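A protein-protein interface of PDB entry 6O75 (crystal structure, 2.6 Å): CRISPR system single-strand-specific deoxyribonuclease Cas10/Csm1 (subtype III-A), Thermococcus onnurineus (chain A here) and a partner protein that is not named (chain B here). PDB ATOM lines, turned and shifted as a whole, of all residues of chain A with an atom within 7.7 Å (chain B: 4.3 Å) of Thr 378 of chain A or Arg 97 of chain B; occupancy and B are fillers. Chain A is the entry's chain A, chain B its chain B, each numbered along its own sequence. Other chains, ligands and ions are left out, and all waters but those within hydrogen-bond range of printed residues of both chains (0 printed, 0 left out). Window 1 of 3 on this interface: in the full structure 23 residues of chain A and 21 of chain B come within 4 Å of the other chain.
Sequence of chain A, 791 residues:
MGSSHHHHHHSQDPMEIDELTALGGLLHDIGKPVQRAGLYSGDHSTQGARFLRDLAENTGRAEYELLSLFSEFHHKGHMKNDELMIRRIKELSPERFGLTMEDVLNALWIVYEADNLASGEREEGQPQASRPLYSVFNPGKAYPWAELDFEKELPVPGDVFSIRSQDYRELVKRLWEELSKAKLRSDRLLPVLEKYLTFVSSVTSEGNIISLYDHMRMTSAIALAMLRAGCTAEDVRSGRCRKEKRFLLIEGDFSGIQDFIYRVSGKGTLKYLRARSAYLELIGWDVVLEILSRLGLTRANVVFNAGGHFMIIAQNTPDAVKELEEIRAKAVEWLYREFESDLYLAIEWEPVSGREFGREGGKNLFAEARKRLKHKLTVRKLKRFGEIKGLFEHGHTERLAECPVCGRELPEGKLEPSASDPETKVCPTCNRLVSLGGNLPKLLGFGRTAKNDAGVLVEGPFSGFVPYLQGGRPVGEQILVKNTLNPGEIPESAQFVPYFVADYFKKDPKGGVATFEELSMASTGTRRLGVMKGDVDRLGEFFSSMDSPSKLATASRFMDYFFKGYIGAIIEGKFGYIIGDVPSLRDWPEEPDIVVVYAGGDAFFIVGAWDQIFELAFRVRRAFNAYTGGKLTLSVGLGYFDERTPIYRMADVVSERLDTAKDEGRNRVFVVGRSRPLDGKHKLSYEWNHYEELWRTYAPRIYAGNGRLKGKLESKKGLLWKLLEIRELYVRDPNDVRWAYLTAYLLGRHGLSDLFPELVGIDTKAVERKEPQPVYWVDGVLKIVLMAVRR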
ATOM      1  N   ALA A 346      11.596  27.473  22.620  1.00  0.00           N
ATOM      2  CA  ALA A 346      12.158  26.270  21.973  1.00  0.00           C
ATOM      3  C   ALA A 346      11.892  26.369  20.470  1.00  0.00           C
ATOM      4  O   ALA A 346      10.710  26.348  20.090  1.00  0.00           O
ATOM      5  CB  ALA A 346      11.542  25.035  22.574  1.00  0.00           C
ATOM      6  N   GLU A 348      12.954  24.671  16.667  1.00  0.00           N
ATOM      7  CA  GLU A 348      13.531  23.530  15.915  1.00  0.00           C
ATOM      8  C   GLU A 348      13.024  23.589  14.472  1.00  0.00           C
ATOM      9  O   GLU A 348      12.035  24.300  14.205  1.00  0.00           O
ATOM     10  CB  GLU A 348      13.166  22.205  16.581  1.00  0.00           C
ATOM     11  CG  GLU A 348      13.948  21.926  17.854  1.00  0.00           C
ATOM     12  CD  GLU A 348      15.428  21.619  17.673  1.00  0.00           C
ATOM     13  OE1 GLU A 348      16.241  22.184  18.432  1.00  0.00           O
ATOM     14  OE2 GLU A 348      15.765  20.808  16.786  1.00  0.00           O
ATOM     15  N   LYS A 371       5.317  14.860  13.559  1.00  0.00           N
ATOM     16  CA  LYS A 371       5.608  14.028  14.761  1.00  0.00           C
ATOM     17  C   LYS A 371       7.113  14.058  15.085  1.00  0.00           C
ATOM     18  O   LYS A 371       7.450  14.223  16.274  1.00  0.00           O
ATOM     19  CB  LYS A 371       5.102  12.600  14.548  1.00  0.00           C
ATOM     20  CG  LYS A 371       4.804  11.814  15.818  1.00  0.00           C
ATOM     21  CD  LYS A 371       3.707  10.778  15.649  1.00  0.00           C
ATOM     22  CE  LYS A 371       3.212  10.214  16.965  1.00  0.00           C
ATOM     23  NZ  LYS A 371       2.136   9.214  16.764  1.00  0.00           N
ATOM     24  N   ARG A 372       7.985  13.903  14.081  1.00  0.00           N
ATOM     25  CA  ARG A 372       9.471  13.928  14.230  1.00  0.00           C
ATOM     26  C   ARG A 372       9.937  15.336  14.627  1.00  0.00           C
ATOM     27  O   ARG A 372      10.984  15.450  15.296  1.00  0.00           O
ATOM     28  CB  ARG A 372      10.179  13.489  12.940  1.00  0.00           C
ATOM     29  CG  ARG A 372      10.150  11.984  12.691  1.00  0.00           C
ATOM     30  CD  ARG A 372      11.175  11.512  11.671  1.00  0.00           C
ATOM     31  NE  ARG A 372      11.248  12.418  10.529  1.00  0.00           N
ATOM     32  CZ  ARG A 372      10.439  12.392   9.469  1.00  0.00           C
ATOM     33  NH1 ARG A 372       9.476  11.489   9.371  1.00  0.00           N
ATOM     34  NH2 ARG A 372      10.600  13.283   8.505  1.00  0.00           N
ATOM     35  N   LEU A 373       9.210  16.376  14.215  1.00  0.00           N
ATOM     36  CA  LEU A 373       9.535  17.777  14.583  1.00  0.00           C
ATOM     37  C   LEU A 373       9.107  18.020  16.037  1.00  0.00           C
ATOM     38  O   LEU A 373       9.890  18.614  16.788  1.00  0.00           O
ATOM     39  CB  LEU A 373       8.833  18.730  13.615  1.00  0.00           C
ATOM     40  CG  LEU A 373       9.059  20.214  13.876  1.00  0.00           C
ATOM     41  CD1 LEU A 373      10.541  20.538  13.979  1.00  0.00           C
ATOM     42  CD2 LEU A 373       8.410  21.044  12.786  1.00  0.00           C
ATOM     43  N   LYS A 374       7.913  17.552  16.408  1.00  0.00           N
ATOM     44  CA  LYS A 374       7.396  17.547  17.803  1.00  0.00           C
ATOM     45  C   LYS A 374       8.468  16.966  18.736  1.00  0.00           C
ATOM     46  O   LYS A 374       8.777  17.612  19.758  1.00  0.00           O
ATOM     47  CB  LYS A 374       6.091  16.746  17.877  1.00  0.00           C
ATOM     48  CG  LYS A 374       5.377  16.788  19.221  1.00  0.00           C
ATOM     49  CD  LYS A 374       4.748  18.131  19.521  1.00  0.00           C
ATOM     50  CE  LYS A 374       5.017  18.614  20.931  1.00  0.00           C
ATOM     51  NZ  LYS A 374       6.303  19.348  21.046  1.00  0.00           N
ATOM     52  N   HIS A 375       9.028  15.804  18.386  1.00  0.00           N
ATOM     53  CA  HIS A 375      10.055  15.090  19.190  1.00  0.00           C
ATOM     54  C   HIS A 375      11.272  15.995  19.407  1.00  0.00           C
ATOM     55  O   HIS A 375      11.777  16.041  20.542  1.00  0.00           O
ATOM     56  CB  HIS A 375      10.467  13.759  18.543  1.00  0.00           C
ATOM     57  CG  HIS A 375      11.427  12.987  19.386  1.00  0.00           C
ATOM     58  ND1 HIS A 375      12.771  12.869  19.065  1.00  0.00           N
ATOM     59  CD2 HIS A 375      11.255  12.343  20.563  1.00  0.00           C
ATOM     60  CE1 HIS A 375      13.380  12.159  19.993  1.00  0.00           C
ATOM     61  NE2 HIS A 375      12.470  11.824  20.924  1.00  0.00           N
ATOM     62  N   LYS A 376      11.748  16.668  18.356  1.00  0.00           N
ATOM     63  CA  LYS A 376      12.925  17.569  18.463  1.00  0.00           C
ATOM     64  C   LYS A 376      12.601  18.680  19.474  1.00  0.00           C
ATOM     65  O   LYS A 376      13.515  19.078  20.220  1.00  0.00           O
ATOM     66  CB  LYS A 376      13.315  18.152  17.100  1.00  0.00           C
ATOM     67  CG  LYS A 376      14.035  17.202  16.150  1.00  0.00           C
ATOM     68  CD  LYS A 376      14.862  17.931  15.100  1.00  0.00           C
ATOM     69  CE  LYS A 376      14.747  17.356  13.702  1.00  0.00           C
ATOM     70  NZ  LYS A 376      15.800  16.351  13.418  1.00  0.00           N
ATOM     71  N   LEU A 377      11.349  19.153  19.504  1.00  0.00           N
ATOM     72  CA  LEU A 377      10.908  20.269  20.384  1.00  0.00           C
ATOM     73  C   LEU A 377      10.900  19.799  21.841  1.00  0.00           C
ATOM     74  O   LEU A 377      11.364  20.564  22.705  1.00  0.00           O
ATOM     75  CB  LEU A 377       9.518  20.757  19.966  1.00  0.00           C
ATOM     76  CG  LEU A 377       9.471  21.769  18.825  1.00  0.00           C
ATOM     77  CD1 LEU A 377       8.037  22.206  18.577  1.00  0.00           C
ATOM     78  CD2 LEU A 377      10.342  22.981  19.109  1.00  0.00           C
ATOM     79  N   THR A 378      10.384  18.597  22.096  1.00  0.00           N
ATOM     80  CA  THR A 378      10.316  17.993  23.449  1.00  0.00           C
ATOM     81  C   THR A 378      11.742  17.862  24.002  1.00  0.00           C
ATOM     82  O   THR A 378      11.940  18.227  25.179  1.00  0.00           O
ATOM     83  CB  THR A 378       9.526  16.680  23.422  1.00  0.00           C
ATOM     84  OG1 THR A 378       9.957  15.944  22.283  1.00  0.00           O
ATOM     85  CG2 THR A 378       8.031  16.889  23.336  1.00  0.00           C
ATOM     86  N   VAL A 379      12.693  17.402  23.177  1.00  0.00           N
ATOM     87  CA  VAL A 379      14.146  17.297  23.520  1.00  0.00           C
ATOM     88  C   VAL A 379      14.684  18.699  23.824  1.00  0.00           C
ATOM     89  O   VAL A 379      15.396  18.845  24.827  1.00  0.00           O
ATOM     90  CB  VAL A 379      14.966  16.631  22.393  1.00  0.00           C
ATOM     91  CG1 VAL A 379      16.463  16.777  22.613  1.00  0.00           C
ATOM     92  CG2 VAL A 379      14.603  15.165  22.209  1.00  0.00           C
ATOM     93  N   ARG A 380      14.376  19.686  22.983  1.00  0.00           N
ATOM     94  CA  ARG A 380      14.893  21.072  23.123  1.00  0.00           C
ATOM     95  C   ARG A 380      14.343  21.687  24.419  1.00  0.00           C
ATOM     96  O   ARG A 380      15.094  22.426  25.087  1.00  0.00           O
ATOM     97  CB  ARG A 380      14.545  21.894  21.876  1.00  0.00           C
ATOM     98  CG  ARG A 380      14.969  23.355  21.921  1.00  0.00           C
ATOM     99  CD  ARG A 380      16.432  23.569  22.243  1.00  0.00           C
ATOM    100  NE  ARG A 380      17.297  23.285  21.111  1.00  0.00           N
ATOM    101  CZ  ARG A 380      18.626  23.250  21.168  1.00  0.00           C
ATOM    102  NH1 ARG A 380      19.254  23.473  22.315  1.00  0.00           N
ATOM    103  NH2 ARG A 380      19.320  22.980  20.074  1.00  0.00           N
ATOM    104  N   LYS A 381      13.101  21.364  24.791  1.00  0.00           N
ATOM    105  CA  LYS A 381      12.467  21.840  26.053  1.00  0.00           C
ATOM    106  C   LYS A 381      13.170  21.232  27.278  1.00  0.00           C
ATOM    107  O   LYS A 381      13.079  21.836  28.362  1.00  0.00           O
ATOM    108  CB  LYS A 381      10.975  21.515  26.063  1.00  0.00           C
ATOM    109  CG  LYS A 381      10.119  22.462  25.238  1.00  0.00           C
ATOM    110  CD  LYS A 381       8.658  22.098  25.243  1.00  0.00           C
ATOM    111  CE  LYS A 381       7.936  22.554  23.994  1.00  0.00           C
ATOM    112  NZ  LYS A 381       6.470  22.575  24.200  1.00  0.00           N
ATOM    113  N   LEU A 382      13.845  20.093  27.105  1.00  0.00           N
ATOM    114  CA  LEU A 382      14.653  19.411  28.151  1.00  0.00           C
ATOM    115  C   LEU A 382      16.120  19.850  28.058  1.00  0.00           C
ATOM    116  O   LEU A 382      16.931  19.297  28.814  1.00  0.00           O
ATOM    117  CB  LEU A 382      14.504  17.895  27.977  1.00  0.00           C
ATOM    118  CG  LEU A 382      13.098  17.340  28.208  1.00  0.00           C
ATOM    119  CD1 LEU A 382      12.999  15.890  27.759  1.00  0.00           C
ATOM    120  CD2 LEU A 382      12.693  17.468  29.668  1.00  0.00           C
ATOM    121  N   LYS A 383      16.449  20.806  27.180  1.00  0.00           N
ATOM    122  CA  LYS A 383      17.796  21.439  27.088  1.00  0.00           C
ATOM    123  C   LYS A 383      17.606  22.958  27.146  1.00  0.00           C
ATOM    124  O   LYS A 383      18.243  23.689  26.358  1.00  0.00           O
ATOM    125  CB  LYS A 383      18.536  20.955  25.834  1.00  0.00           C
ATOM    126  CG  LYS A 383      18.696  19.439  25.724  1.00  0.00           C
ATOM    127  CD  LYS A 383      18.996  18.940  24.323  1.00  0.00           C
ATOM    128  CE  LYS A 383      20.475  18.916  23.995  1.00  0.00           C
ATOM    129  NZ  LYS A 383      21.122  17.680  24.496  1.00  0.00           N
ATOM    130  N   ARG A 384      16.756  23.392  28.077  1.00  0.00           N
ATOM    131  CA  ARG A 384      16.329  24.798  28.302  1.00  0.00           C
ATOM    132  C   ARG A 384      17.536  25.720  28.470  1.00  0.00           C
ATOM    133  O   ARG A 384      18.292  25.536  29.442  1.00  0.00           O
ATOM    134  CB  ARG A 384      15.497  24.898  29.581  1.00  0.00           C
ATOM    135  CG  ARG A 384      14.011  25.105  29.358  1.00  0.00           C
ATOM    136  CD  ARG A 384      13.536  26.157  30.337  1.00  0.00           C
ATOM    137  NE  ARG A 384      12.089  26.281  30.352  1.00  0.00           N
ATOM    138  CZ  ARG A 384      11.438  27.225  31.007  1.00  0.00           C
ATOM    139  NH1 ARG A 384      10.120  27.266  30.974  1.00  0.00           N
ATOM    140  NH2 ARG A 384      12.103  28.128  31.701  1.00  0.00           N
ATOM    141  N   GLU B  74      11.290  10.817  29.096  1.00  0.00           N
ATOM    142  CA  GLU B  74      10.327  11.823  28.563  1.00  0.00           C
ATOM    143  C   GLU B  74      10.295  11.726  27.038  1.00  0.00           C
ATOM    144  O   GLU B  74       9.218  11.618  26.455  1.00  0.00           O
ATOM    145  CB  GLU B  74      10.672  13.254  28.988  1.00  0.00           C
ATOM    146  CG  GLU B  74      10.771  13.474  30.489  1.00  0.00           C
ATOM    147  CD  GLU B  74       9.464  13.836  31.169  1.00  0.00           C
ATOM    148  OE1 GLU B  74       8.525  13.039  31.071  1.00  0.00           O
ATOM    149  OE2 GLU B  74       9.394  14.915  31.787  1.00  0.00           O
ATOM    150  N   LEU B  77       8.956   7.845  25.315  1.00  0.00           N
ATOM    151  CA  LEU B  77       7.673   7.238  25.779  1.00  0.00           C
ATOM    152  C   LEU B  77       7.024   6.352  24.701  1.00  0.00           C
ATOM    153  O   LEU B  77       6.295   5.418  25.090  1.00  0.00           O
ATOM    154  CB  LEU B  77       6.718   8.348  26.230  1.00  0.00           C
ATOM    155  CG  LEU B  77       7.093   9.039  27.542  1.00  0.00           C
ATOM    156  CD1 LEU B  77       6.354  10.358  27.703  1.00  0.00           C
ATOM    157  CD2 LEU B  77       6.830   8.136  28.740  1.00  0.00           C
ATOM    158  N   ALA B  93       0.771   8.945  28.206  1.00  0.00           N
ATOM    159  CA  ALA B  93       2.034   9.672  27.919  1.00  0.00           C
ATOM    160  C   ALA B  93       2.019  11.077  28.536  1.00  0.00           C
ATOM    161  O   ALA B  93       3.103  11.546  28.925  1.00  0.00           O
ATOM    162  CB  ALA B  93       2.266   9.746  26.431  1.00  0.00           C
ATOM    163  N   LYS B  94       0.852  11.729  28.596  1.00  0.00           N
ATOM    164  CA  LYS B  94       0.679  13.072  29.217  1.00  0.00           C
ATOM    165  C   LYS B  94       0.795  12.948  30.746  1.00  0.00           C
ATOM    166  O   LYS B  94       1.325  13.896  31.356  1.00  0.00           O
ATOM    167  CB  LYS B  94      -0.656  13.701  28.798  1.00  0.00           C
ATOM    168  CG  LYS B  94      -0.798  15.194  29.083  1.00  0.00           C
ATOM    169  CD  LYS B  94      -0.240  16.103  27.995  1.00  0.00           C
ATOM    170  CE  LYS B  94      -1.305  16.847  27.209  1.00  0.00           C
ATOM    171  NZ  LYS B  94      -2.060  15.961  26.290  1.00  0.00           N
ATOM    172  N   ARG B  95       0.342  11.830  31.333  1.00  0.00           N
ATOM    173  CA  ARG B  95       0.345  11.583  32.808  1.00  0.00           C
ATOM    174  C   ARG B  95       1.696  11.015  33.267  1.00  0.00           C
ATOM    175  O   ARG B  95       2.077  11.281  34.426  1.00  0.00           O
ATOM    176  CB  ARG B  95      -0.823  10.677  33.223  1.00  0.00           C
ATOM    177  CG  ARG B  95      -2.012  11.429  33.815  1.00  0.00           C
ATOM    178  CD  ARG B  95      -2.242  12.763  33.117  1.00  0.00           C
ATOM    179  NE  ARG B  95      -3.494  13.456  33.404  1.00  0.00           N
ATOM    180  CZ  ARG B  95      -3.925  14.530  32.736  1.00  0.00           C
ATOM    181  NH1 ARG B  95      -3.215  15.025  31.735  1.00  0.00           N
ATOM    182  NH2 ARG B  95      -5.071  15.106  33.054  1.00  0.00           N
ATOM    183  N   LEU B  96       2.398  10.272  32.409  1.00  0.00           N
ATOM    184  CA  LEU B  96       3.800   9.850  32.671  1.00  0.00           C
ATOM    185  C   LEU B  96       4.667  11.114  32.648  1.00  0.00           C
ATOM    186  O   LEU B  96       5.528  11.257  33.527  1.00  0.00           O
ATOM    187  CB  LEU B  96       4.278   8.832  31.626  1.00  0.00           C
ATOM    188  CG  LEU B  96       3.392   7.605  31.366  1.00  0.00           C
ATOM    189  CD1 LEU B  96       4.242   6.386  31.024  1.00  0.00           C
ATOM    190  CD2 LEU B  96       2.485   7.278  32.542  1.00  0.00           C
ATOM    191  N   ARG B  97       4.395  12.016  31.701  1.00  0.00           N
ATOM    192  CA  ARG B  97       5.146  13.282  31.481  1.00  0.00           C
ATOM    193  C   ARG B  97       4.966  14.219  32.684  1.00  0.00           C
ATOM    194  O   ARG B  97       5.876  15.036  32.923  1.00  0.00           O
ATOM    195  CB  ARG B  97       4.689  13.943  30.174  1.00  0.00           C
ATOM    196  CG  ARG B  97       5.595  15.061  29.674  1.00  0.00           C
ATOM    197  CD  ARG B  97       5.061  15.730  28.419  1.00  0.00           C
ATOM    198  NE  ARG B  97       5.074  14.863  27.243  1.00  0.00           N
ATOM    199  CZ  ARG B  97       6.150  14.572  26.510  1.00  0.00           C
ATOM    200  NH1 ARG B  97       6.034  13.778  25.459  1.00  0.00           N
ATOM    201  NH2 ARG B  97       7.338  15.063  26.826  1.00  0.00           N
ATOM    202  N   LYS B  98       3.844  14.110  33.408  1.00  0.00           N
ATOM    203  CA  LYS B  98       3.492  14.981  34.567  1.00  0.00           C
ATOM    204  C   LYS B  98       4.003  14.368  35.879  1.00  0.00           C
ATOM    205  O   LYS B  98       4.233  15.141  36.832  1.00  0.00           O
ATOM    206  CB  LYS B  98       1.977  15.217  34.624  1.00  0.00           C
ATOM    207  CG  LYS B  98       1.447  16.225  33.609  1.00  0.00           C
ATOM    208  CD  LYS B  98      -0.069  16.300  33.528  1.00  0.00           C
ATOM    209  CE  LYS B  98      -0.555  17.410  32.619  1.00  0.00           C
ATOM    210  NZ  LYS B  98      -1.941  17.829  32.942  1.00  0.00           N
ATOM    211  N   ALA B  99       4.175  13.041  35.932  1.00  0.00           N
ATOM    212  CA  ALA B  99       4.652  12.297  37.123  1.00  0.00           C
ATOM    213  C   ALA B  99       6.036  12.809  37.545  1.00  0.00           C
ATOM    214  O   ALA B  99       6.922  12.951  36.671  1.00  0.00           O
ATOM    215  CB  ALA B  99       4.686  10.820  36.834  1.00  0.00           C
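The backbone carbonyl oxygen of His 375 of chain A sits at hydrogen-bond distance from the side-chain hydroxyl of Thr 378 of chain A (2.5 Å).
The backbone carbonyl oxygen (O) of Lys 374 of chain A lies within hydrogen-bond range of the side-chain hydroxyl (OG1) of Thr 378 of chain A (3.2 Å).
Arg 97 of chain B touches Thr 378 of chain A (NH2 to CG2, 3.999 Å).
CD1 of Leu 382 of chain A touches CB of Glu 74 of chain B, 3.7 Å away.
Of the printed residues of chain B, Thr 378 of chain A touches Arg 97 (3.999 Å).
Of the printed residues of chain B, Leu 382 of chain A touches Glu 74 (3.7 Å).
Of the printed residues of chain A, Glu 74 of chain B touches Leu 382.
Of the printed residues of chain A, Arg 97 of chain B touches Thr 378 (3.999 Å).
The nearest printed residue of chain A that does not touch Arg 97 of chain B is Leu 382 of chain A (5.8 Å).
Of the 16 printed residues of chain A, 2 touch a printed residue of chain B.
Of the 9 printed residues of chain B, 2 touch a printed residue of chain A.
Printed residues of chain B that touch a printed residue of chain A: Glu 74 and Arg 97.
Among the printed residues, no Asp or Glu carboxylate lies within 4 Å of a Lys or Arg side-chain nitrogen of the other chain.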
